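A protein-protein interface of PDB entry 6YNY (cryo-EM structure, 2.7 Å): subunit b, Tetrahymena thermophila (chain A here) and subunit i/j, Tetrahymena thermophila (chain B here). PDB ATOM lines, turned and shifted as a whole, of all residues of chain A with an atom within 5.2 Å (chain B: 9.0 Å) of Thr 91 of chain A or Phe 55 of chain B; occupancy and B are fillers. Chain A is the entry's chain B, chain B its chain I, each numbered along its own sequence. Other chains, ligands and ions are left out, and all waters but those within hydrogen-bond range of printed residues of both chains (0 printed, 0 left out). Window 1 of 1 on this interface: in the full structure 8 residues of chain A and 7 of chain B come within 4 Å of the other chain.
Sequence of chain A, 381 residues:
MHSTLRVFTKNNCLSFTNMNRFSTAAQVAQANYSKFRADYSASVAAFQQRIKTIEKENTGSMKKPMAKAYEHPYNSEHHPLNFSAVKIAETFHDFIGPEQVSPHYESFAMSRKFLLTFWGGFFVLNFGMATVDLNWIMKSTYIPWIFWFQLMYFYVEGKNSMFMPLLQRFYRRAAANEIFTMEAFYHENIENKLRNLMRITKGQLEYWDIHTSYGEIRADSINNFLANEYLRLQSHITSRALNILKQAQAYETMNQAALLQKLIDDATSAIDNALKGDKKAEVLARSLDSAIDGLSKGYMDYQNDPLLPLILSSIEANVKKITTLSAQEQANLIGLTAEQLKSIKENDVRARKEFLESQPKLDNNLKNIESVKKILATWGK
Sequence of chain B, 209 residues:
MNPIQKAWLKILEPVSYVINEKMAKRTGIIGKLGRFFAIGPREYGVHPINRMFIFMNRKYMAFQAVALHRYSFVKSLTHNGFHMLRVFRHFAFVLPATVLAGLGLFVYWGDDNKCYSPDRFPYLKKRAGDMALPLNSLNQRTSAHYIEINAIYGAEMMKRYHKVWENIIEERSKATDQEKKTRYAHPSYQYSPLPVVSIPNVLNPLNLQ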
ATOM      1  N   LYS A  87      10.558 -23.064 -15.102  1.00  0.00           N
ATOM      2  CA  LYS A  87      10.895 -23.692 -16.374  1.00  0.00           C
ATOM      3  C   LYS A  87      10.069 -23.106 -17.510  1.00  0.00           C
ATOM      4  O   LYS A  87      10.562 -22.964 -18.633  1.00  0.00           O
ATOM      5  CB  LYS A  87      10.691 -25.202 -16.289  1.00  0.00           C
ATOM      6  CG  LYS A  87      11.137 -25.959 -17.524  1.00  0.00           C
ATOM      7  CD  LYS A  87      12.638 -25.952 -17.666  1.00  0.00           C
ATOM      8  CE  LYS A  87      13.079 -26.579 -18.965  1.00  0.00           C
ATOM      9  NZ  LYS A  87      14.557 -26.616 -19.056  1.00  0.00           N
ATOM     10  N   ILE A  88       8.810 -22.765 -17.236  1.00  0.00           N
ATOM     11  CA  ILE A  88       7.984 -22.110 -18.243  1.00  0.00           C
ATOM     12  C   ILE A  88       8.590 -20.771 -18.634  1.00  0.00           C
ATOM     13  O   ILE A  88       8.555 -20.373 -19.803  1.00  0.00           O
ATOM     14  CB  ILE A  88       6.545 -21.951 -17.721  1.00  0.00           C
ATOM     15  CG1 ILE A  88       5.948 -23.317 -17.393  1.00  0.00           C
ATOM     16  CG2 ILE A  88       5.684 -21.240 -18.735  1.00  0.00           C
ATOM     17  CD1 ILE A  88       4.618 -23.244 -16.705  1.00  0.00           C
ATOM     18  N   ALA A  89       9.155 -20.056 -17.662  1.00  0.00           N
ATOM     19  CA  ALA A  89       9.813 -18.792 -17.963  1.00  0.00           C
ATOM     20  C   ALA A  89      11.057 -19.005 -18.809  1.00  0.00           C
ATOM     21  O   ALA A  89      11.360 -18.199 -19.694  1.00  0.00           O
ATOM     22  CB  ALA A  89      10.165 -18.072 -16.667  1.00  0.00           C
ATOM     23  N   GLU A  90      11.792 -20.086 -18.549  1.00  0.00           N
ATOM     24  CA  GLU A  90      12.971 -20.389 -19.349  1.00  0.00           C
ATOM     25  C   GLU A  90      12.593 -20.662 -20.797  1.00  0.00           C
ATOM     26  O   GLU A  90      13.275 -20.205 -21.720  1.00  0.00           O
ATOM     27  CB  GLU A  90      13.708 -21.581 -18.745  1.00  0.00           C
ATOM     28  CG  GLU A  90      15.089 -21.812 -19.308  1.00  0.00           C
ATOM     29  CD  GLU A  90      15.670 -23.149 -18.898  1.00  0.00           C
ATOM     30  OE1 GLU A  90      15.217 -24.184 -19.427  1.00  0.00           O
ATOM     31  OE2 GLU A  90      16.583 -23.169 -18.048  1.00  0.00           O
ATOM     32  N   THR A  91      11.505 -21.403 -21.016  1.00  0.00           N
ATOM     33  CA  THR A  91      11.065 -21.684 -22.376  1.00  0.00           C
ATOM     34  C   THR A  91      10.450 -20.458 -23.029  1.00  0.00           C
ATOM     35  O   THR A  91      10.550 -20.289 -24.247  1.00  0.00           O
ATOM     36  CB  THR A  91      10.060 -22.832 -22.387  1.00  0.00           C
ATOM     37  OG1 THR A  91       8.890 -22.456 -21.655  1.00  0.00           O
ATOM     38  CG2 THR A  91      10.654 -24.061 -21.770  1.00  0.00           C
ATOM     39  N   PHE A  92       9.806 -19.599 -22.240  1.00  0.00           N
ATOM     40  CA  PHE A  92       9.198 -18.400 -22.798  1.00  0.00           C
ATOM     41  C   PHE A  92      10.253 -17.454 -23.351  1.00  0.00           C
ATOM     42  O   PHE A  92      10.089 -16.906 -24.446  1.00  0.00           O
ATOM     43  CB  PHE A  92       8.357 -17.706 -21.732  1.00  0.00           C
ATOM     44  CG  PHE A  92       7.745 -16.421 -22.182  1.00  0.00           C
ATOM     45  CD1 PHE A  92       8.218 -15.216 -21.715  1.00  0.00           C
ATOM     46  CD2 PHE A  92       6.698 -16.416 -23.078  1.00  0.00           C
ATOM     47  CE1 PHE A  92       7.659 -14.040 -22.126  1.00  0.00           C
ATOM     48  CE2 PHE A  92       6.139 -15.239 -23.490  1.00  0.00           C
ATOM     49  CZ  PHE A  92       6.621 -14.050 -23.014  1.00  0.00           C
ATOM     50  N   HIS A  93      11.344 -17.255 -22.615  1.00  0.00           N
ATOM     51  CA  HIS A  93      12.380 -16.338 -23.066  1.00  0.00           C
ATOM     52  C   HIS A  93      13.221 -16.928 -24.186  1.00  0.00           C
ATOM     53  O   HIS A  93      13.759 -16.179 -25.007  1.00  0.00           O
ATOM     54  CB  HIS A  93      13.260 -15.921 -21.892  1.00  0.00           C
ATOM     55  CG  HIS A  93      12.646 -14.858 -21.038  1.00  0.00           C
ATOM     56  ND1 HIS A  93      11.837 -15.142 -19.962  1.00  0.00           N
ATOM     57  CD2 HIS A  93      12.706 -13.508 -21.118  1.00  0.00           C
ATOM     58  CE1 HIS A  93      11.433 -14.014 -19.408  1.00  0.00           C
ATOM     59  NE2 HIS A  93      11.945 -13.007 -20.092  1.00  0.00           N
ATOM     60  N   ASP A  94      13.347 -18.252 -24.247  1.00  0.00           N
ATOM     61  CA  ASP A  94      13.942 -18.865 -25.425  1.00  0.00           C
ATOM     62  C   ASP A  94      13.105 -18.585 -26.663  1.00  0.00           C
ATOM     63  O   ASP A  94      13.645 -18.477 -27.769  1.00  0.00           O
ATOM     64  CB  ASP A  94      14.088 -20.370 -25.225  1.00  0.00           C
ATOM     65  CG  ASP A  94      14.987 -20.725 -24.060  1.00  0.00           C
ATOM     66  OD1 ASP A  94      15.559 -19.804 -23.441  1.00  0.00           O
ATOM     67  OD2 ASP A  94      15.121 -21.929 -23.760  1.00  0.00           O
ATOM     68  N   PHE A  95      11.791 -18.454 -26.494  1.00  0.00           N
ATOM     69  CA  PHE A  95      10.893 -18.228 -27.618  1.00  0.00           C
ATOM     70  C   PHE A  95      10.923 -16.776 -28.082  1.00  0.00           C
ATOM     71  O   PHE A  95      11.202 -16.496 -29.252  1.00  0.00           O
ATOM     72  CB  PHE A  95       9.479 -18.664 -27.230  1.00  0.00           C
ATOM     73  CG  PHE A  95       8.405 -18.098 -28.097  1.00  0.00           C
ATOM     74  CD1 PHE A  95       7.343 -17.421 -27.537  1.00  0.00           C
ATOM     75  CD2 PHE A  95       8.453 -18.236 -29.468  1.00  0.00           C
ATOM     76  CE1 PHE A  95       6.352 -16.898 -28.323  1.00  0.00           C
ATOM     77  CE2 PHE A  95       7.464 -17.713 -30.260  1.00  0.00           C
ATOM     78  CZ  PHE A  95       6.411 -17.041 -29.686  1.00  0.00           C
ATOM     79  N   PRO B  48      12.110 -20.005 -33.991  1.00  0.00           N
ATOM     80  CA  PRO B  48      11.060 -19.625 -33.035  1.00  0.00           C
ATOM     81  C   PRO B  48       9.866 -20.561 -33.001  1.00  0.00           C
ATOM     82  O   PRO B  48       9.218 -20.668 -31.953  1.00  0.00           O
ATOM     83  CB  PRO B  48      10.666 -18.221 -33.509  1.00  0.00           C
ATOM     84  CG  PRO B  48      11.855 -17.719 -34.198  1.00  0.00           C
ATOM     85  CD  PRO B  48      12.475 -18.884 -34.866  1.00  0.00           C
ATOM     86  N   ILE B  49       9.541 -21.236 -34.102  1.00  0.00           N
ATOM     87  CA  ILE B  49       8.399 -22.146 -34.096  1.00  0.00           C
ATOM     88  C   ILE B  49       8.659 -23.320 -33.161  1.00  0.00           C
ATOM     89  O   ILE B  49       7.788 -23.715 -32.379  1.00  0.00           O
ATOM     90  CB  ILE B  49       8.076 -22.620 -35.522  1.00  0.00           C
ATOM     91  CG1 ILE B  49       7.540 -21.458 -36.343  1.00  0.00           C
ATOM     92  CG2 ILE B  49       7.052 -23.733 -35.492  1.00  0.00           C
ATOM     93  CD1 ILE B  49       7.392 -21.766 -37.797  1.00  0.00           C
ATOM     94  N   ASN B  50       9.852 -23.906 -33.242  1.00  0.00           N
ATOM     95  CA  ASN B  50      10.228 -24.949 -32.296  1.00  0.00           C
ATOM     96  C   ASN B  50      10.088 -24.456 -30.864  1.00  0.00           C
ATOM     97  O   ASN B  50       9.522 -25.141 -30.008  1.00  0.00           O
ATOM     98  CB  ASN B  50      11.661 -25.404 -32.555  1.00  0.00           C
ATOM     99  CG  ASN B  50      11.839 -26.041 -33.908  1.00  0.00           C
ATOM    100  OD1 ASN B  50      10.957 -25.976 -34.760  1.00  0.00           O
ATOM    101  ND2 ASN B  50      12.994 -26.661 -34.115  1.00  0.00           N
ATOM    102  N   ARG B  51      10.605 -23.261 -30.591  1.00  0.00           N
ATOM    103  CA  ARG B  51      10.530 -22.710 -29.246  1.00  0.00           C
ATOM    104  C   ARG B  51       9.095 -22.408 -28.844  1.00  0.00           C
ATOM    105  O   ARG B  51       8.717 -22.603 -27.684  1.00  0.00           O
ATOM    106  CB  ARG B  51      11.375 -21.447 -29.157  1.00  0.00           C
ATOM    107  CG  ARG B  51      12.736 -21.637 -28.530  1.00  0.00           C
ATOM    108  CD  ARG B  51      13.722 -22.277 -29.462  1.00  0.00           C
ATOM    109  NE  ARG B  51      15.081 -22.111 -28.966  1.00  0.00           N
ATOM    110  CZ  ARG B  51      16.160 -22.629 -29.538  1.00  0.00           C
ATOM    111  NH1 ARG B  51      16.056 -23.359 -30.642  1.00  0.00           N
ATOM    112  NH2 ARG B  51      17.347 -22.412 -28.998  1.00  0.00           N
ATOM    113  N   MET B  52       8.285 -21.916 -29.779  1.00  0.00           N
ATOM    114  CA  MET B  52       6.889 -21.641 -29.467  1.00  0.00           C
ATOM    115  C   MET B  52       6.180 -22.901 -28.990  1.00  0.00           C
ATOM    116  O   MET B  52       5.363 -22.852 -28.066  1.00  0.00           O
ATOM    117  CB  MET B  52       6.184 -21.062 -30.690  1.00  0.00           C
ATOM    118  CG  MET B  52       4.857 -20.412 -30.384  1.00  0.00           C
ATOM    119  SD  MET B  52       3.833 -20.123 -31.837  1.00  0.00           S
ATOM    120  CE  MET B  52       4.819 -18.924 -32.710  1.00  0.00           C
ATOM    121  N   PHE B  53       6.482 -24.040 -29.612  1.00  0.00           N
ATOM    122  CA  PHE B  53       5.908 -25.305 -29.169  1.00  0.00           C
ATOM    123  C   PHE B  53       6.407 -25.688 -27.783  1.00  0.00           C
ATOM    124  O   PHE B  53       5.618 -26.104 -26.927  1.00  0.00           O
ATOM    125  CB  PHE B  53       6.241 -26.403 -30.174  1.00  0.00           C
ATOM    126  CG  PHE B  53       6.134 -27.782 -29.613  1.00  0.00           C
ATOM    127  CD1 PHE B  53       4.921 -28.432 -29.567  1.00  0.00           C
ATOM    128  CD2 PHE B  53       7.250 -28.430 -29.128  1.00  0.00           C
ATOM    129  CE1 PHE B  53       4.825 -29.695 -29.048  1.00  0.00           C
ATOM    130  CE2 PHE B  53       7.156 -29.691 -28.607  1.00  0.00           C
ATOM    131  CZ  PHE B  53       5.943 -30.325 -28.567  1.00  0.00           C
ATOM    132  N   ILE B  54       7.709 -25.553 -27.544  1.00  0.00           N
ATOM    133  CA  ILE B  54       8.283 -25.950 -26.264  1.00  0.00           C
ATOM    134  C   ILE B  54       7.662 -25.149 -25.129  1.00  0.00           C
ATOM    135  O   ILE B  54       7.396 -25.680 -24.046  1.00  0.00           O
ATOM    136  CB  ILE B  54       9.813 -25.791 -26.302  1.00  0.00           C
ATOM    137  CG1 ILE B  54      10.414 -26.763 -27.315  1.00  0.00           C
ATOM    138  CG2 ILE B  54      10.399 -26.010 -24.933  1.00  0.00           C
ATOM    139  CD1 ILE B  54      11.856 -26.508 -27.624  1.00  0.00           C
ATOM    140  N   PHE B  55       7.417 -23.860 -25.360  1.00  0.00           N
ATOM    141  CA  PHE B  55       6.824 -23.022 -24.327  1.00  0.00           C
ATOM    142  C   PHE B  55       5.359 -23.371 -24.105  1.00  0.00           C
ATOM    143  O   PHE B  55       4.922 -23.564 -22.966  1.00  0.00           O
ATOM    144  CB  PHE B  55       6.981 -21.551 -24.701  1.00  0.00           C
ATOM    145  CG  PHE B  55       6.056 -20.637 -23.965  1.00  0.00           C
ATOM    146  CD1 PHE B  55       6.080 -20.566 -22.588  1.00  0.00           C
ATOM    147  CD2 PHE B  55       5.163 -19.841 -24.651  1.00  0.00           C
ATOM    148  CE1 PHE B  55       5.230 -19.731 -21.916  1.00  0.00           C
ATOM    149  CE2 PHE B  55       4.315 -19.004 -23.981  1.00  0.00           C
ATOM    150  CZ  PHE B  55       4.347 -18.947 -22.613  1.00  0.00           C
ATOM    151  N   MET B  56       4.582 -23.457 -25.184  1.00  0.00           N
ATOM    152  CA  MET B  56       3.161 -23.748 -25.053  1.00  0.00           C
ATOM    153  C   MET B  56       2.915 -25.177 -24.593  1.00  0.00           C
ATOM    154  O   MET B  56       1.941 -25.436 -23.880  1.00  0.00           O
ATOM    155  CB  MET B  56       2.460 -23.486 -26.381  1.00  0.00           C
ATOM    156  CG  MET B  56       2.601 -22.056 -26.869  1.00  0.00           C
ATOM    157  SD  MET B  56       1.965 -20.836 -25.712  1.00  0.00           S
ATOM    158  CE  MET B  56       0.264 -21.355 -25.612  1.00  0.00           C
ATOM    159  N   ASN B  57       3.774 -26.112 -24.993  1.00  0.00           N
ATOM    160  CA  ASN B  57       3.677 -27.472 -24.480  1.00  0.00           C
ATOM    161  C   ASN B  57       3.838 -27.501 -22.969  1.00  0.00           C
ATOM    162  O   ASN B  57       3.085 -28.186 -22.268  1.00  0.00           O
ATOM    163  CB  ASN B  57       4.733 -28.348 -25.148  1.00  0.00           C
ATOM    164  CG  ASN B  57       4.945 -29.661 -24.434  1.00  0.00           C
ATOM    165  OD1 ASN B  57       5.846 -29.793 -23.611  1.00  0.00           O
ATOM    166  ND2 ASN B  57       4.118 -30.641 -24.746  1.00  0.00           N
ATOM    167  N   ARG B  58       4.807 -26.749 -22.448  1.00  0.00           N
ATOM    168  CA  ARG B  58       5.076 -26.763 -21.017  1.00  0.00           C
ATOM    169  C   ARG B  58       3.970 -26.066 -20.237  1.00  0.00           C
ATOM    170  O   ARG B  58       3.570 -26.531 -19.165  1.00  0.00           O
ATOM    171  CB  ARG B  58       6.427 -26.106 -20.746  1.00  0.00           C
ATOM    172  CG  ARG B  58       6.959 -26.299 -19.351  1.00  0.00           C
ATOM    173  CD  ARG B  58       7.522 -27.684 -19.155  1.00  0.00           C
ATOM    174  NE  ARG B  58       7.684 -28.005 -17.743  1.00  0.00           N
ATOM    175  CZ  ARG B  58       8.121 -29.172 -17.288  1.00  0.00           C
ATOM    176  NH1 ARG B  58       8.447 -30.137 -18.130  1.00  0.00           N
ATOM    177  NH2 ARG B  58       8.233 -29.374 -15.987  1.00  0.00           N
ATOM    178  N   LYS B  59       3.466 -24.947 -20.757  1.00  0.00           N
ATOM    179  CA  LYS B  59       2.431 -24.203 -20.050  1.00  0.00           C
ATOM    180  C   LYS B  59       1.114 -24.968 -20.032  1.00  0.00           C
ATOM    181  O   LYS B  59       0.422 -24.997 -19.010  1.00  0.00           O
ATOM    182  CB  LYS B  59       2.255 -22.827 -20.690  1.00  0.00           C
ATOM    183  CG  LYS B  59       1.425 -21.867 -19.876  1.00  0.00           C
ATOM    184  CD  LYS B  59       1.491 -20.467 -20.430  1.00  0.00           C
ATOM    185  CE  LYS B  59       0.932 -19.452 -19.454  1.00  0.00           C
ATOM    186  NZ  LYS B  59      -0.523 -19.565 -19.294  1.00  0.00           N
ATOM    187  N   TYR B  60       0.750 -25.591 -21.152  1.00  0.00           N
ATOM    188  CA  TYR B  60      -0.484 -26.364 -21.195  1.00  0.00           C
ATOM    189  C   TYR B  60      -0.370 -27.640 -20.377  1.00  0.00           C
ATOM    190  O   TYR B  60      -1.371 -28.121 -19.837  1.00  0.00           O
ATOM    191  CB  TYR B  60      -0.843 -26.691 -22.641  1.00  0.00           C
ATOM    192  CG  TYR B  60      -2.077 -27.543 -22.788  1.00  0.00           C
ATOM    193  CD1 TYR B  60      -1.975 -28.900 -23.022  1.00  0.00           C
ATOM    194  CD2 TYR B  60      -3.340 -26.992 -22.692  1.00  0.00           C
ATOM    195  CE1 TYR B  60      -3.092 -29.680 -23.156  1.00  0.00           C
ATOM    196  CE2 TYR B  60      -4.463 -27.767 -22.826  1.00  0.00           C
ATOM    197  CZ  TYR B  60      -4.334 -29.112 -23.058  1.00  0.00           C
ATOM    198  OH  TYR B  60      -5.452 -29.895 -23.191  1.00  0.00           O
ATOM    199  N   MET B  61       0.836 -28.192 -20.262  1.00  0.00           N
ATOM    200  CA  MET B  61       1.015 -29.410 -19.488  1.00  0.00           C
ATOM    201  C   MET B  61       0.882 -29.143 -17.995  1.00  0.00           C
ATOM    202  O   MET B  61       0.325 -29.964 -17.259  1.00  0.00           O
ATOM    203  CB  MET B  61       2.374 -30.022 -19.799  1.00  0.00           C
ATOM    204  CG  MET B  61       2.526 -31.409 -19.278  1.00  0.00           C
ATOM    205  SD  MET B  61       3.921 -32.299 -19.958  1.00  0.00           S
ATOM    206  CE  MET B  61       3.441 -33.923 -19.411  1.00  0.00           C
ATOM    207  N   ALA B  62       1.394 -28.005 -17.529  1.00  0.00           N
ATOM    208  CA  ALA B  62       1.199 -27.631 -16.136  1.00  0.00           C
ATOM    209  C   ALA B  62      -0.277 -27.476 -15.804  1.00  0.00           C
ATOM    210  O   ALA B  62      -0.680 -27.685 -14.656  1.00  0.00           O
ATOM    211  CB  ALA B  62       1.951 -26.338 -15.837  1.00  0.00           C
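OG1 of Thr 91 of chain A sits at hydrogen-bond distance from O of Ile 88 of chain A, at 2.8 Å. O of Lys 87 of chain A sits close to OG1 of Thr 91 of chain A (3.5 Å).
Among the printed residues, pairs that only touch across the chains: Ile 88 of chain A with Phe 55 of chain B, Ile 88 of chain A with Arg 58 of chain B, Thr 91 of chain A with Ile 54 of chain B, Thr 91 of chain A with Phe 55 of chain B, Phe 92 of chain A with Phe 55 of chain B, Asp 94 of chain A with Arg 51 of chain B, Phe 95 of chain A with Pro 48 of chain B, Phe 95 of chain A with Arg 51 of chain B and Phe 95 of chain A with Met 52 of chain B.
Thr 91 of chain A touches just these residues of chain B: Ile 54 (3.7 Å) and Phe 55 (3.4 Å). Of the printed residues of chain A, Phe 55 of chain B touches Ile 88 (3.5 Å), Thr 91 (3.4 Å) and Phe 92 (3.5 Å). Of the printed residues of chain B, Asp 94 of chain A touches Arg 51 (3.4 Å). Of the printed residues of chain A, Ile 54 of chain B touches Thr 91. The nearest printed residue of chain A that does not touch Met 52 of chain B is Thr 91 of chain A (6.2 Å).
Hydrophobic or aromatic side chains of chain A that line the printed part of chain B: Ile 88, Phe 92 and Phe 95. Printed residues of chain B that touch a printed residue of chain A: Pro 48, Arg 51, Met 52, Ile 54, Phe 55 and Arg 58. Hydrophobic or aromatic side chains of chain B that line the printed part of chain A: Met 52, Ile 54 and Phe 55. Among the printed residues, 9 pairs touch across the chains.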
